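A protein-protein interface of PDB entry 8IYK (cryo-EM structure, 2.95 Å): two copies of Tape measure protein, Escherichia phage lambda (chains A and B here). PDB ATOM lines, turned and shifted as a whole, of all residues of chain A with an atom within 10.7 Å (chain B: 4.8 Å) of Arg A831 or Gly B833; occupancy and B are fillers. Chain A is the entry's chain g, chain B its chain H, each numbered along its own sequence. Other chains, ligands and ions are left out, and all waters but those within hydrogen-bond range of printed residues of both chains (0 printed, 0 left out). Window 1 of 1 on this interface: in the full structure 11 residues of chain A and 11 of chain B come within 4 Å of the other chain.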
ATOM      1  N   LEU A 823     -18.200   3.785  24.086  1.00  0.00           N
ATOM      2  CA  LEU A 823     -17.302   2.816  23.463  1.00  0.00           C
ATOM      3  C   LEU A 823     -16.050   3.489  22.911  1.00  0.00           C
ATOM      4  O   LEU A 823     -14.947   2.944  23.027  1.00  0.00           O
ATOM      5  CB  LEU A 823     -18.035   2.048  22.364  1.00  0.00           C
ATOM      6  CG  LEU A 823     -18.914   0.890  22.842  1.00  0.00           C
ATOM      7  CD1 LEU A 823     -19.127  -0.118  21.727  1.00  0.00           C
ATOM      8  CD2 LEU A 823     -18.313   0.215  24.066  1.00  0.00           C
ATOM      9  N   LYS A 824     -16.196   4.672  22.310  1.00  0.00           N
ATOM     10  CA  LYS A 824     -15.026   5.400  21.826  1.00  0.00           C
ATOM     11  C   LYS A 824     -14.104   5.793  22.972  1.00  0.00           C
ATOM     12  O   LYS A 824     -12.875   5.688  22.857  1.00  0.00           O
ATOM     13  CB  LYS A 824     -15.464   6.639  21.049  1.00  0.00           C
ATOM     14  CG  LYS A 824     -14.350   7.308  20.262  1.00  0.00           C
ATOM     15  CD  LYS A 824     -13.554   6.307  19.448  1.00  0.00           C
ATOM     16  CE  LYS A 824     -12.391   6.984  18.744  1.00  0.00           C
ATOM     17  NZ  LYS A 824     -12.620   8.443  18.566  1.00  0.00           N
ATOM     18  N   ALA A 825     -14.677   6.255  24.085  1.00  0.00           N
ATOM     19  CA  ALA A 825     -13.860   6.612  25.238  1.00  0.00           C
ATOM     20  C   ALA A 825     -13.120   5.399  25.784  1.00  0.00           C
ATOM     21  O   ALA A 825     -11.938   5.488  26.135  1.00  0.00           O
ATOM     22  CB  ALA A 825     -14.731   7.244  26.323  1.00  0.00           C
ATOM     23  N   VAL A 826     -13.801   4.253  25.859  1.00  0.00           N
ATOM     24  CA  VAL A 826     -13.154   3.040  26.350  1.00  0.00           C
ATOM     25  C   VAL A 826     -12.033   2.617  25.410  1.00  0.00           C
ATOM     26  O   VAL A 826     -10.949   2.223  25.851  1.00  0.00           O
ATOM     27  CB  VAL A 826     -14.190   1.918  26.547  1.00  0.00           C
ATOM     28  CG1 VAL A 826     -13.499   0.613  26.894  1.00  0.00           C
ATOM     29  CG2 VAL A 826     -15.173   2.295  27.639  1.00  0.00           C
ATOM     30  N   TYR A 827     -12.270   2.704  24.098  1.00  0.00           N
ATOM     31  CA  TYR A 827     -11.240   2.347  23.127  1.00  0.00           C
ATOM     32  C   TYR A 827     -10.019   3.248  23.251  1.00  0.00           C
ATOM     33  O   TYR A 827      -8.878   2.775  23.196  1.00  0.00           O
ATOM     34  CB  TYR A 827     -11.816   2.420  21.715  1.00  0.00           C
ATOM     35  CG  TYR A 827     -10.861   1.979  20.631  1.00  0.00           C
ATOM     36  CD1 TYR A 827     -10.554   0.639  20.451  1.00  0.00           C
ATOM     37  CD2 TYR A 827     -10.274   2.906  19.783  1.00  0.00           C
ATOM     38  CE1 TYR A 827      -9.684   0.237  19.458  1.00  0.00           C
ATOM     39  CE2 TYR A 827      -9.404   2.513  18.790  1.00  0.00           C
ATOM     40  CZ  TYR A 827      -9.113   1.179  18.632  1.00  0.00           C
ATOM     41  OH  TYR A 827      -8.244   0.785  17.640  1.00  0.00           O
ATOM     42  N   ASP A 828     -10.236   4.552  23.419  1.00  0.00           N
ATOM     43  CA  ASP A 828      -9.105   5.471  23.497  1.00  0.00           C
ATOM     44  C   ASP A 828      -8.349   5.317  24.813  1.00  0.00           C
ATOM     45  O   ASP A 828      -7.116   5.421  24.844  1.00  0.00           O
ATOM     46  CB  ASP A 828      -9.590   6.903  23.308  1.00  0.00           C
ATOM     47  CG  ASP A 828     -10.043   7.176  21.886  1.00  0.00           C
ATOM     48  OD1 ASP A 828     -10.551   6.240  21.238  1.00  0.00           O
ATOM     49  OD2 ASP A 828      -9.888   8.319  21.410  1.00  0.00           O
ATOM     50  N   MET A 829      -9.067   5.064  25.908  1.00  0.00           N
ATOM     51  CA  MET A 829      -8.394   4.763  27.168  1.00  0.00           C
ATOM     52  C   MET A 829      -7.596   3.471  27.060  1.00  0.00           C
ATOM     53  O   MET A 829      -6.506   3.357  27.630  1.00  0.00           O
ATOM     54  CB  MET A 829      -9.415   4.675  28.302  1.00  0.00           C
ATOM     55  CG  MET A 829      -8.811   4.348  29.655  1.00  0.00           C
ATOM     56  SD  MET A 829      -8.175   5.792  30.522  1.00  0.00           S
ATOM     57  CE  MET A 829      -9.698   6.570  31.041  1.00  0.00           C
ATOM     58  N   ALA A 830      -8.122   2.488  26.327  1.00  0.00           N
ATOM     59  CA  ALA A 830      -7.373   1.261  26.077  1.00  0.00           C
ATOM     60  C   ALA A 830      -6.110   1.539  25.276  1.00  0.00           C
ATOM     61  O   ALA A 830      -5.055   0.956  25.545  1.00  0.00           O
ATOM     62  CB  ALA A 830      -8.255   0.251  25.348  1.00  0.00           C
ATOM     63  N   ARG A 831      -6.202   2.417  24.274  1.00  0.00           N
ATOM     64  CA  ARG A 831      -5.021   2.795  23.503  1.00  0.00           C
ATOM     65  C   ARG A 831      -3.970   3.443  24.396  1.00  0.00           C
ATOM     66  O   ARG A 831      -2.777   3.121  24.312  1.00  0.00           O
ATOM     67  CB  ARG A 831      -5.420   3.745  22.374  1.00  0.00           C
ATOM     68  CG  ARG A 831      -6.072   3.073  21.182  1.00  0.00           C
ATOM     69  CD  ARG A 831      -5.060   2.288  20.372  1.00  0.00           C
ATOM     70  NE  ARG A 831      -5.201   2.538  18.943  1.00  0.00           N
ATOM     71  CZ  ARG A 831      -4.427   3.357  18.245  1.00  0.00           C
ATOM     72  NH1 ARG A 831      -3.440   4.028  18.815  1.00  0.00           N
ATOM     73  NH2 ARG A 831      -4.650   3.509  16.943  1.00  0.00           N
ATOM     74  N   LYS A 832      -4.399   4.365  25.260  1.00  0.00           N
ATOM     75  CA  LYS A 832      -3.462   5.022  26.167  1.00  0.00           C
ATOM     76  C   LYS A 832      -2.828   4.022  27.125  1.00  0.00           C
ATOM     77  O   LYS A 832      -1.619   4.075  27.380  1.00  0.00           O
ATOM     78  CB  LYS A 832      -4.166   6.132  26.944  1.00  0.00           C
ATOM     79  CG  LYS A 832      -3.250   7.273  27.352  1.00  0.00           C
ATOM     80  CD  LYS A 832      -2.688   7.062  28.747  1.00  0.00           C
ATOM     81  CE  LYS A 832      -1.617   8.086  29.075  1.00  0.00           C
ATOM     82  NZ  LYS A 832      -0.623   8.221  27.976  1.00  0.00           N
ATOM     83  N   GLY A 833      -3.631   3.108  27.671  1.00  0.00           N
ATOM     84  CA  GLY A 833      -3.086   2.098  28.562  1.00  0.00           C
ATOM     85  C   GLY A 833      -2.101   1.182  27.865  1.00  0.00           C
ATOM     86  O   GLY A 833      -1.078   0.805  28.438  1.00  0.00           O
ATOM     87  N   ALA A 834      -2.394   0.814  26.617  1.00  0.00           N
ATOM     88  CA  ALA A 834      -1.476  -0.021  25.853  1.00  0.00           C
ATOM     89  C   ALA A 834      -0.161   0.698  25.597  1.00  0.00           C
ATOM     90  O   ALA A 834       0.914   0.101  25.720  1.00  0.00           O
ATOM     91  CB  ALA A 834      -2.124  -0.442  24.536  1.00  0.00           C
ATOM     92  N   ARG A 835      -0.223   1.982  25.240  1.00  0.00           N
ATOM     93  CA  ARG A 835       1.006   2.743  25.032  1.00  0.00           C
ATOM     94  C   ARG A 835       1.813   2.850  26.321  1.00  0.00           C
ATOM     95  O   ARG A 835       3.041   2.690  26.311  1.00  0.00           O
ATOM     96  CB  ARG A 835       0.682   4.132  24.485  1.00  0.00           C
ATOM     97  CG  ARG A 835       1.548   4.547  23.310  1.00  0.00           C
ATOM     98  CD  ARG A 835       0.883   5.637  22.491  1.00  0.00           C
ATOM     99  NE  ARG A 835      -0.080   6.401  23.276  1.00  0.00           N
ATOM    100  CZ  ARG A 835      -1.340   6.606  22.919  1.00  0.00           C
ATOM    101  NH1 ARG A 835      -1.827   6.117  21.791  1.00  0.00           N
ATOM    102  NH2 ARG A 835      -2.131   7.324  23.712  1.00  0.00           N
ATOM    103  N   ASP A 836       1.140   3.113  27.443  1.00  0.00           N
ATOM    104  CA  ASP A 836       1.839   3.206  28.721  1.00  0.00           C
ATOM    105  C   ASP A 836       2.480   1.878  29.099  1.00  0.00           C
ATOM    106  O   ASP A 836       3.620   1.844  29.575  1.00  0.00           O
ATOM    107  CB  ASP A 836       0.876   3.665  29.813  1.00  0.00           C
ATOM    108  CG  ASP A 836       0.592   5.148  29.751  1.00  0.00           C
ATOM    109  OD1 ASP A 836       0.819   5.753  28.682  1.00  0.00           O
ATOM    110  OD2 ASP A 836       0.140   5.709  30.770  1.00  0.00           O
ATOM    111  N   GLU A 837       1.764   0.771  28.893  1.00  0.00           N
ATOM    112  CA  GLU A 837       2.320  -0.541  29.202  1.00  0.00           C
ATOM    113  C   GLU A 837       3.511  -0.859  28.307  1.00  0.00           C
ATOM    114  O   GLU A 837       4.510  -1.423  28.768  1.00  0.00           O
ATOM    115  CB  GLU A 837       1.240  -1.611  29.061  1.00  0.00           C
ATOM    116  CG  GLU A 837       1.641  -2.970  29.596  1.00  0.00           C
ATOM    117  CD  GLU A 837       1.490  -3.065  31.099  1.00  0.00           C
ATOM    118  OE1 GLU A 837       2.386  -2.584  31.823  1.00  0.00           O
ATOM    119  OE2 GLU A 837       0.469  -3.616  31.561  1.00  0.00           O
ATOM    120  N   ILE A 838       3.424  -0.504  27.024  1.00  0.00           N
ATOM    121  CA  ILE A 838       4.544  -0.729  26.115  1.00  0.00           C
ATOM    122  C   ILE A 838       5.766   0.046  26.585  1.00  0.00           C
ATOM    123  O   ILE A 838       6.869  -0.501  26.677  1.00  0.00           O
ATOM    124  CB  ILE A 838       4.156  -0.350  24.675  1.00  0.00           C
ATOM    125  CG1 ILE A 838       3.267  -1.431  24.059  1.00  0.00           C
ATOM    126  CG2 ILE A 838       5.397  -0.139  23.827  1.00  0.00           C
ATOM    127  CD1 ILE A 838       2.529  -0.980  22.821  1.00  0.00           C
ATOM    128  N   GLN A 839       5.583   1.327  26.912  1.00  0.00           N
ATOM    129  CA  GLN A 839       6.712   2.125  27.385  1.00  0.00           C
ATOM    130  C   GLN A 839       7.257   1.599  28.706  1.00  0.00           C
ATOM    131  O   GLN A 839       8.460   1.707  28.967  1.00  0.00           O
ATOM    132  CB  GLN A 839       6.307   3.592  27.521  1.00  0.00           C
ATOM    133  CG  GLN A 839       5.794   4.210  26.236  1.00  0.00           C
ATOM    134  CD  GLN A 839       6.484   5.515  25.903  1.00  0.00           C
ATOM    135  OE1 GLN A 839       7.711   5.602  25.916  1.00  0.00           O
ATOM    136  NE2 GLN A 839       5.696   6.541  25.604  1.00  0.00           N
ATOM    137  N   MET B 829     -12.401  -4.840  24.588  1.00  0.00           N
ATOM    138  CA  MET B 829     -12.044  -3.575  23.958  1.00  0.00           C
ATOM    139  C   MET B 829     -10.591  -3.218  24.243  1.00  0.00           C
ATOM    140  O   MET B 829      -9.890  -2.692  23.373  1.00  0.00           O
ATOM    141  CB  MET B 829     -12.974  -2.464  24.443  1.00  0.00           C
ATOM    142  CG  MET B 829     -12.623  -1.091  23.904  1.00  0.00           C
ATOM    143  SD  MET B 829     -13.394  -0.745  22.313  1.00  0.00           S
ATOM    144  CE  MET B 829     -15.031  -1.410  22.592  1.00  0.00           C
ATOM    145  N   ALA B 830     -10.122  -3.500  25.461  1.00  0.00           N
ATOM    146  CA  ALA B 830      -8.724  -3.258  25.798  1.00  0.00           C
ATOM    147  C   ALA B 830      -7.795  -4.139  24.976  1.00  0.00           C
ATOM    148  O   ALA B 830      -6.734  -3.688  24.535  1.00  0.00           O
ATOM    149  CB  ALA B 830      -8.501  -3.492  27.290  1.00  0.00           C
ATOM    150  N   ARG B 831      -8.168  -5.404  24.777  1.00  0.00           N
ATOM    151  CA  ARG B 831      -7.367  -6.287  23.934  1.00  0.00           C
ATOM    152  C   ARG B 831      -7.287  -5.758  22.507  1.00  0.00           C
ATOM    153  O   ARG B 831      -6.207  -5.741  21.899  1.00  0.00           O
ATOM    154  CB  ARG B 831      -7.955  -7.697  23.948  1.00  0.00           C
ATOM    155  CG  ARG B 831      -7.788  -8.437  25.262  1.00  0.00           C
ATOM    156  CD  ARG B 831      -6.332  -8.765  25.532  1.00  0.00           C
ATOM    157  NE  ARG B 831      -5.836  -9.797  24.631  1.00  0.00           N
ATOM    158  CZ  ARG B 831      -5.917 -11.099  24.868  1.00  0.00           C
ATOM    159  NH1 ARG B 831      -6.471 -11.567  25.974  1.00  0.00           N
ATOM    160  NH2 ARG B 831      -5.430 -11.953  23.973  1.00  0.00           N
ATOM    161  N   LYS B 832      -8.422  -5.320  21.958  1.00  0.00           N
ATOM    162  CA  LYS B 832      -8.422  -4.765  20.606  1.00  0.00           C
ATOM    163  C   LYS B 832      -7.567  -3.507  20.526  1.00  0.00           C
ATOM    164  O   LYS B 832      -6.810  -3.322  19.566  1.00  0.00           O
ATOM    165  CB  LYS B 832      -9.848  -4.467  20.154  1.00  0.00           C
ATOM    166  CG  LYS B 832     -10.045  -4.568  18.652  1.00  0.00           C
ATOM    167  CD  LYS B 832      -9.885  -3.214  17.982  1.00  0.00           C
ATOM    168  CE  LYS B 832      -9.966  -3.333  16.472  1.00  0.00           C
ATOM    169  NZ  LYS B 832      -9.038  -4.373  15.955  1.00  0.00           N
ATOM    170  N   GLY B 833      -7.679  -2.629  21.522  1.00  0.00           N
ATOM    171  CA  GLY B 833      -6.866  -1.425  21.530  1.00  0.00           C
ATOM    172  C   GLY B 833      -5.384  -1.726  21.632  1.00  0.00           C
ATOM    173  O   GLY B 833      -4.562  -1.070  20.991  1.00  0.00           O
ATOM    174  N   ALA B 834      -5.024  -2.722  22.444  1.00  0.00           N
ATOM    175  CA  ALA B 834      -3.625  -3.115  22.559  1.00  0.00           C
ATOM    176  C   ALA B 834      -3.097  -3.661  21.242  1.00  0.00           C
ATOM    177  O   ALA B 834      -1.979  -3.333  20.831  1.00  0.00           O
ATOM    178  CB  ALA B 834      -3.462  -4.147  23.672  1.00  0.00           C
ATOM    179  N   ARG B 835      -3.887  -4.495  20.562  1.00  0.00           N
ATOM    180  CA  ARG B 835      -3.460  -5.007  19.263  1.00  0.00           C
ATOM    181  C   ARG B 835      -3.298  -3.880  18.252  1.00  0.00           C
ATOM    182  O   ARG B 835      -2.324  -3.855  17.487  1.00  0.00           O
ATOM    183  CB  ARG B 835      -4.456  -6.044  18.748  1.00  0.00           C
ATOM    184  CG  ARG B 835      -3.820  -7.357  18.336  1.00  0.00           C
ATOM    185  CD  ARG B 835      -4.776  -8.516  18.538  1.00  0.00           C
ATOM    186  NE  ARG B 835      -6.167  -8.087  18.490  1.00  0.00           N
ATOM    187  CZ  ARG B 835      -7.097  -8.466  19.357  1.00  0.00           C
ATOM    188  NH1 ARG B 835      -6.817  -9.285  20.356  1.00  0.00           N
ATOM    189  NH2 ARG B 835      -8.338  -8.011  19.215  1.00  0.00           N
ATOM    190  N   ASP B 836      -4.242  -2.937  18.233  1.00  0.00           N
ATOM    191  CA  ASP B 836      -4.149  -1.812  17.307  1.00  0.00           C
ATOM    192  C   ASP B 836      -2.920  -0.959  17.595  1.00  0.00           C
ATOM    193  O   ASP B 836      -2.211  -0.548  16.671  1.00  0.00           O
ATOM    194  CB  ASP B 836      -5.415  -0.964  17.386  1.00  0.00           C
ATOM    195  CG  ASP B 836      -6.554  -1.544  16.576  1.00  0.00           C
ATOM    196  OD1 ASP B 836      -6.598  -2.781  16.412  1.00  0.00           O
ATOM    197  OD2 ASP B 836      -7.405  -0.761  16.106  1.00  0.00           O
ATOM    198  N   GLU B 837      -2.649  -0.688  18.873  1.00  0.00           N
ATOM    199  CA  GLU B 837      -1.481   0.108  19.231  1.00  0.00           C
ATOM    200  C   GLU B 837      -0.190  -0.612  18.865  1.00  0.00           C
ATOM    201  O   GLU B 837       0.760   0.011  18.377  1.00  0.00           O
ATOM    202  CB  GLU B 837      -1.511   0.436  20.721  1.00  0.00           C
ATOM    203  CG  GLU B 837      -0.494   1.476  21.144  1.00  0.00           C
ATOM    204  CD  GLU B 837      -0.963   2.890  20.862  1.00  0.00           C
ATOM    205  OE1 GLU B 837      -0.862   3.331  19.699  1.00  0.00           O
ATOM    206  OE2 GLU B 837      -1.441   3.557  21.803  1.00  0.00           O
ATOM    207  N   THR B 840       0.300  -0.351  15.257  1.00  0.00           N
ATOM    208  CA  THR B 840       0.663   1.018  14.909  1.00  0.00           C
ATOM    209  C   THR B 840       2.138   1.286  15.180  1.00  0.00           C
ATOM    210  O   THR B 840       2.811   1.948  14.382  1.00  0.00           O
ATOM    211  CB  THR B 840      -0.214   2.002  15.683  1.00  0.00           C
ATOM    212  OG1 THR B 840      -1.567   1.902  15.222  1.00  0.00           O
ATOM    213  CG2 THR B 840       0.272   3.426  15.490  1.00  0.00           C
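Leu A823 touches Met B829.
Met B829 touches Val A826 (CG to CG1, 3.6 Å).
CB of Tyr A827 touches SD of Met B829, 3.6 Å away.
Tyr A827 touches Lys B832 (CE1 to CD, 3.8 Å).
CE1 of Tyr A827 touches CA of Gly B833 (3.9 Å).
Ala B830 touches Ala A830 (CA to CB, 3.6 Å).
Arg A831 touches Gly B833.
Arg A831 touches Asp B836 (NE to CB, 3.8 Å).
Arg A831 touches Thr B840.
Ala A834 touches Ala B834 (CB to CA, 3.6 Å).
Ala B830 touches its own counterpart, Ala A830.
Arg A831 touches Gly B833, but with the chains exchanged Gly A833 does not touch Arg B831 (9.5 Å).
Ala A834 touches its own counterpart, Ala B834.
Arg A835 touches Glu B837, but with the chains exchanged Glu A837 does not touch Arg B835 (10.3 Å).
Positions printed for both chains: 829, 830, 831, 832, 833, 834, 835, 836 and 837.
Of the 15 pairs that touch across the chains among the printed residues, 2 have their exchanged pair printed and touching as well.
Of chain A, only Tyr A827 (3.9 Å) and Arg A831 (3.5 Å) come within 4 Å of Gly B833.
Ala B830 touches just one residue of chain A: Ala A830.
Of chain A, only Ala A834 (3.6 Å) comes within 4 Å of Ala B834.
Of the printed residues of chain A, Asp B836 touches Tyr A827 and Arg A831.
Glu B837 touches just these residues of chain A: Arg A831 (2.8 Å), Ala A834 (3.96 Å) and Arg A835 (2.6 Å).
Of the printed residues of chain B, Arg A835 touches Glu B837.
Of the printed residues of chain A, Thr B840 touches Arg A831.
Of the printed residues of chain B, Val A826 touches Met B829.
Of the printed residues of chain B, Ala A834 touches Ala B834 and Glu B837.
Printed residues of chain B within 4 Å of Tyr A827: Met B829, Lys B832, Gly B833 and Asp B836.
Glu A837 touches none of the printed residues of chain B.
The nearest printed residue of chain B that does not touch Tyr A827 is Glu B837 (5.9 Å).
The side-chain carboxylate (OE1) of Glu B837 is in salt-bridge range of the guanidinium group (NH1) of Arg A831 (2.8 Å).
The side-chain carboxylate of Glu B837 lies within salt-bridge range of the guanidinium group of Arg A835.
The side-chain carboxylate (OD2) of Asp B836 sits close to the side-chain hydroxyl (OH) of Tyr A827 (2.3 Å).
The side-chain amino group (NZ) of Lys B832 is in salt-bridge range of the side-chain carboxylate (OD1) of Asp B836, 2.9 Å away.
O of Asp B836 lies within hydrogen-bond range of OG1 of Thr B840 (2.9 Å).
Printed residues of chain A that touch a printed residue of chain B: Leu A823, Val A826, Tyr A827, Ala A830, Arg A831, Ala A834 and Arg A835.
Hydrophobic or aromatic side chains of chain A within 4 Å of the printed part of chain B: Leu A823, Val A826, Tyr A827, Ala A830 and Ala A834.
Of the 10 printed residues of chain B, 8 touch a printed residue of chain A.
Hydrophobic or aromatic side chains of chain B that line the printed part of chain A: Met B829.
Among the printed residues, Asp or Glu carboxylates within 4 Å of a Lys or Arg side-chain nitrogen of the other chain: Arg A831 with Glu B837 (2.8 Å) and Arg A835 with Glu B837 (2.6 Å).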
